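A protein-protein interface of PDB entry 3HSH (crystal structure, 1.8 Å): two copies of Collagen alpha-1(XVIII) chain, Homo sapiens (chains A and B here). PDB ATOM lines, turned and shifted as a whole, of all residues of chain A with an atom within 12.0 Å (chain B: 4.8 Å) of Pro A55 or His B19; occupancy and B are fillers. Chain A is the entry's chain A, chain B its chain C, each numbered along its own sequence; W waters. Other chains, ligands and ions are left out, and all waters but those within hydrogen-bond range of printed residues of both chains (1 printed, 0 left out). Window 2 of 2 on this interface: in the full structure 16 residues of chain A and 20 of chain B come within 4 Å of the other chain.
The backbone carbonyl oxygen of Val B18 is in hydrogen-bond range of the guanidinium group of Arg B38 (2.9 Å).
The backbone carbonyl oxygen of His B19 lies within hydrogen-bond range of the guanidinium group of Arg B38, at 3.2 Å.
The backbone carbonyl oxygen (O) of Val B21 sits at hydrogen-bond distance from the guanidinium group (NE) of Arg B38.
Val B18 touches Leu A54 (CG1 to CD2, 3.8 Å).
NE2 of His B19 touches CB of Leu A54 (3.9 Å).
Arg B38 touches Leu A54 (CZ to CD2, 3.7 Å).
Pro A55 touches Leu B15.
Pro A55 touches Val B18 (CD to CG1, 3.4 Å).
Pro A55 touches His B19.
Of chain B, only Leu B15 (3.4 Å), Val B18 (3.4 Å) and His B19 (3.0 Å) come within 4 Å of Pro A55.
His B19 touches two residues of chain A.
Leu B15 touches one residue of chain A.
Printed residues of chain A within 4 Å of Val B18: Leu A54 and Pro A55.
No residue of chain A comes within 4 Å of Glu B20.
Of the printed residues of chain A, Arg B38 touches Leu A54.
Of the printed residues of chain B, Leu A54 touches Val B18 (3.8 Å), His B19 (3.9 Å) and Arg B38 (3.7 Å).
Pro A53 touches none of the printed residues of chain B.
The nearest printed residue of chain B that does not touch Pro A55 is Gln B17 (6.8 Å).
The nearest printed residue of chain A that does not touch Arg B38 is Thr A52 (7.4 Å).
Of the 7 printed residues of chain B, 4 touch a printed residue of chain A.
Of the 6 printed residues of chain A, 2 touch a printed residue of chain B.
Hydrophobic or aromatic side chains of chain A within 4 Å of the printed part of chain B: Leu A54 and Pro A55.
Among the printed residues, 6 pairs touch across the chains.
Among the printed residues, no Asp or Glu carboxylate lies within 4 Å of a Lys or Arg side-chain nitrogen of the other chain.
No position is printed for both chains.
Of the 6 pairs that touch across the chains among the printed residues, none has its exchanged pair printed and touching as well.
Water W1 lies within hydrogen-bond range of the backbone carbonyl oxygen of Pro A55 (2.7 Å) and a ring nitrogen (NE2) of His B19 (2.9 Å).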
ATOM      1  N   ARG A  51     -15.711 -34.821  31.905  1.00  0.00           N
ATOM      2  CA  ARG A  51     -15.904 -33.999  30.706  1.00  0.00           C
ATOM      3  C   ARG A  51     -16.801 -32.781  30.939  1.00  0.00           C
ATOM      4  O   ARG A  51     -17.914 -32.884  31.505  1.00  0.00           O
ATOM      5  CB  ARG A  51     -16.469 -34.823  29.540  1.00  0.00           C
ATOM      6  CG  ARG A  51     -16.968 -33.948  28.365  1.00  0.00           C
ATOM      7  CD  ARG A  51     -17.604 -34.768  27.261  1.00  0.00           C
ATOM      8  NE  ARG A  51     -18.855 -35.360  27.729  1.00  0.00           N
ATOM      9  CZ  ARG A  51     -20.052 -34.815  27.570  1.00  0.00           C
ATOM     10  NH1 ARG A  51     -20.192 -33.661  26.928  1.00  0.00           N
ATOM     11  NH2 ARG A  51     -21.120 -35.434  28.055  1.00  0.00           N
ATOM     12  N   THR A  52     -16.304 -31.614  30.515  1.00  0.00           N
ATOM     13  CA  THR A  52     -17.073 -30.368  30.480  1.00  0.00           C
ATOM     14  C   THR A  52     -17.678 -30.261  29.077  1.00  0.00           C
ATOM     15  O   THR A  52     -16.948 -30.355  28.094  1.00  0.00           O
ATOM     16  CB  THR A  52     -16.141 -29.148  30.710  1.00  0.00           C
ATOM     17  OG1 THR A  52     -15.522 -29.228  32.011  1.00  0.00           O
ATOM     18  CG2 THR A  52     -16.913 -27.822  30.587  1.00  0.00           C
ATOM     19  N   PRO A  53     -19.013 -30.091  28.969  1.00  0.00           N
ATOM     20  CA  PRO A  53     -19.628 -30.014  27.634  1.00  0.00           C
ATOM     21  C   PRO A  53     -19.165 -28.790  26.859  1.00  0.00           C
ATOM     22  O   PRO A  53     -18.779 -27.781  27.449  1.00  0.00           O
ATOM     23  CB  PRO A  53     -21.142 -29.897  27.938  1.00  0.00           C
ATOM     24  CG  PRO A  53     -21.289 -30.446  29.333  1.00  0.00           C
ATOM     25  CD  PRO A  53     -20.021 -30.052  30.047  1.00  0.00           C
ATOM     26  N   LEU A  54     -19.203 -28.877  25.530  1.00  0.00           N
ATOM     27  CA  LEU A  54     -18.919 -27.715  24.702  1.00  0.00           C
ATOM     28  C   LEU A  54     -20.038 -26.679  24.894  1.00  0.00           C
ATOM     29  O   LEU A  54     -21.191 -27.042  25.113  1.00  0.00           O
ATOM     30  CB  LEU A  54     -18.837 -28.122  23.231  1.00  0.00           C
ATOM     31  CG  LEU A  54     -17.707 -29.094  22.870  1.00  0.00           C
ATOM     32  CD1 LEU A  54     -17.885 -29.584  21.437  1.00  0.00           C
ATOM     33  CD2 LEU A  54     -16.333 -28.434  23.068  1.00  0.00           C
ATOM     34  N   PRO A  55     -19.690 -25.384  24.803  1.00  0.00           N
ATOM     35  CA  PRO A  55     -20.655 -24.301  25.022  1.00  0.00           C
ATOM     36  C   PRO A  55     -21.792 -24.388  24.027  1.00  0.00           C
ATOM     37  O   PRO A  55     -21.608 -24.898  22.913  1.00  0.00           O
ATOM     38  CB  PRO A  55     -19.838 -23.032  24.747  1.00  0.00           C
ATOM     39  CG  PRO A  55     -18.440 -23.445  24.776  1.00  0.00           C
ATOM     40  CD  PRO A  55     -18.380 -24.879  24.380  1.00  0.00           C
ATOM     41  N   ARG A  56     -22.959 -23.897  24.436  1.00  0.00           N
ATOM     42  CA  ARG A  56     -24.155 -23.901  23.619  1.00  0.00           C
ATOM     43  C   ARG A  56     -24.028 -22.909  22.463  1.00  0.00           C
ATOM     44  O   ARG A  56     -23.177 -22.009  22.475  1.00  0.00           O
ATOM     45  CB  ARG A  56     -25.370 -23.559  24.500  1.00  0.00           C
ATOM     46  CG  ARG A  56     -25.494 -24.463  25.742  1.00  0.00           C
ATOM     47  CD  ARG A  56     -26.340 -23.837  26.862  1.00  0.00           C
ATOM     48  NE  ARG A  56     -25.585 -22.905  27.695  1.00  0.00           N
ATOM     49  CZ  ARG A  56     -26.114 -21.887  28.371  1.00  0.00           C
ATOM     50  NH1 ARG A  56     -27.416 -21.641  28.297  1.00  0.00           N
ATOM     51  NH2 ARG A  56     -25.333 -21.100  29.113  1.00  0.00           N
ATOM     52  OXT ARG A  56     -24.768 -23.003  21.482  1.00  0.00           O
ATOM     53  N   LEU B  15     -13.785 -20.369  25.221  1.00  0.00           N
ATOM     54  CA  LEU B  15     -15.102 -20.949  24.970  1.00  0.00           C
ATOM     55  C   LEU B  15     -15.625 -20.604  23.581  1.00  0.00           C
ATOM     56  O   LEU B  15     -16.352 -21.397  22.973  1.00  0.00           O
ATOM     57  CB  LEU B  15     -16.105 -20.543  26.058  1.00  0.00           C
ATOM     58  CG  LEU B  15     -15.856 -21.178  27.437  1.00  0.00           C
ATOM     59  CD1 LEU B  15     -16.824 -20.656  28.476  1.00  0.00           C
ATOM     60  CD2 LEU B  15     -15.923 -22.713  27.333  1.00  0.00           C
ATOM     61  N   GLN B  17     -13.860 -20.377  20.834  1.00  0.00           N
ATOM     62  CA  GLN B  17     -13.158 -21.084  19.764  1.00  0.00           C
ATOM     63  C   GLN B  17     -13.088 -22.590  19.956  1.00  0.00           C
ATOM     64  O   GLN B  17     -12.612 -23.316  19.066  1.00  0.00           O
ATOM     65  CB  GLN B  17     -11.741 -20.553  19.636  1.00  0.00           C
ATOM     66  CG  GLN B  17     -11.713 -19.047  19.405  1.00  0.00           C
ATOM     67  CD  GLN B  17     -10.529 -18.612  18.583  1.00  0.00           C
ATOM     68  OE1 GLN B  17      -9.526 -18.143  19.118  1.00  0.00           O
ATOM     69  NE2 GLN B  17     -10.634 -18.769  17.265  1.00  0.00           N
ATOM     70  N   VAL B  18     -13.545 -23.062  21.107  1.00  0.00           N
ATOM     71  CA  VAL B  18     -13.308 -24.469  21.469  1.00  0.00           C
ATOM     72  C   VAL B  18     -13.937 -25.494  20.492  1.00  0.00           C
ATOM     73  O   VAL B  18     -13.371 -26.575  20.280  1.00  0.00           O
ATOM     74  CB  VAL B  18     -13.690 -24.743  22.960  1.00  0.00           C
ATOM     75  CG1 VAL B  18     -15.212 -24.769  23.152  1.00  0.00           C
ATOM     76  CG2 VAL B  18     -13.055 -26.048  23.472  1.00  0.00           C
ATOM     77  N   HIS B  19     -15.082 -25.168  19.884  1.00  0.00           N
ATOM     78  CA  HIS B  19     -15.682 -26.072  18.885  1.00  0.00           C
ATOM     79  C   HIS B  19     -14.690 -26.419  17.771  1.00  0.00           C
ATOM     80  O   HIS B  19     -14.687 -27.539  17.263  1.00  0.00           O
ATOM     81  CB  HIS B  19     -16.955 -25.469  18.261  1.00  0.00           C
ATOM     82  CG  HIS B  19     -18.192 -25.666  19.085  1.00  0.00           C
ATOM     83  ND1 HIS B  19     -18.545 -24.819  20.118  1.00  0.00           N
ATOM     84  CD2 HIS B  19     -19.166 -26.606  19.024  1.00  0.00           C
ATOM     85  CE1 HIS B  19     -19.678 -25.234  20.660  1.00  0.00           C
ATOM     86  NE2 HIS B  19     -20.080 -26.313  20.009  1.00  0.00           N
ATOM     87  N   GLU B  20     -13.835 -25.461  17.416  1.00  0.00           N
ATOM     88  CA  GLU B  20     -12.926 -25.608  16.279  1.00  0.00           C
ATOM     89  C   GLU B  20     -11.578 -26.218  16.660  1.00  0.00           C
ATOM     90  O   GLU B  20     -10.696 -26.371  15.806  1.00  0.00           O
ATOM     91  CB  GLU B  20     -12.684 -24.248  15.623  1.00  0.00           C
ATOM     92  CG  GLU B  20     -13.916 -23.624  14.971  1.00  0.00           C
ATOM     93  CD  GLU B  20     -13.833 -22.095  14.915  1.00  0.00           C
ATOM     94  OE1 GLU B  20     -13.758 -21.451  15.990  1.00  0.00           O
ATOM     95  OE2 GLU B  20     -13.846 -21.536  13.796  1.00  0.00           O
ATOM     96  N   VAL B  21     -11.386 -26.522  17.942  1.00  0.00           N
ATOM     97  CA  VAL B  21     -10.173 -27.215  18.377  1.00  0.00           C
ATOM     98  C   VAL B  21     -10.431 -28.718  18.263  1.00  0.00           C
ATOM     99  O   VAL B  21     -11.421 -29.207  18.795  1.00  0.00           O
ATOM    100  CB  VAL B  21      -9.853 -26.876  19.856  1.00  0.00           C
ATOM    101  CG1 VAL B  21      -8.591 -27.598  20.334  1.00  0.00           C
ATOM    102  CG2 VAL B  21      -9.700 -25.358  20.012  1.00  0.00           C
ATOM    103  N   ARG B  38      -8.956 -31.486  24.879  1.00  0.00           N
ATOM    104  CA  ARG B  38     -10.164 -31.546  24.055  1.00  0.00           C
ATOM    105  C   ARG B  38     -10.507 -33.011  23.810  1.00  0.00           C
ATOM    106  O   ARG B  38      -9.641 -33.799  23.428  1.00  0.00           O
ATOM    107  CB  ARG B  38      -9.895 -30.834  22.731  1.00  0.00           C
ATOM    108  CG  ARG B  38     -11.154 -30.638  21.842  1.00  0.00           C
ATOM    109  CD  ARG B  38     -12.211 -29.685  22.441  1.00  0.00           C
ATOM    110  NE  ARG B  38     -13.050 -29.288  21.309  1.00  0.00           N
ATOM    111  CZ  ARG B  38     -13.933 -30.080  20.722  1.00  0.00           C
ATOM    112  NH1 ARG B  38     -14.198 -31.272  21.233  1.00  0.00           N
ATOM    113  NH2 ARG B  38     -14.599 -29.659  19.651  1.00  0.00           N
HETATM  114  O   HOH W   1     -22.831 -26.007  20.821  1.00  0.00           O
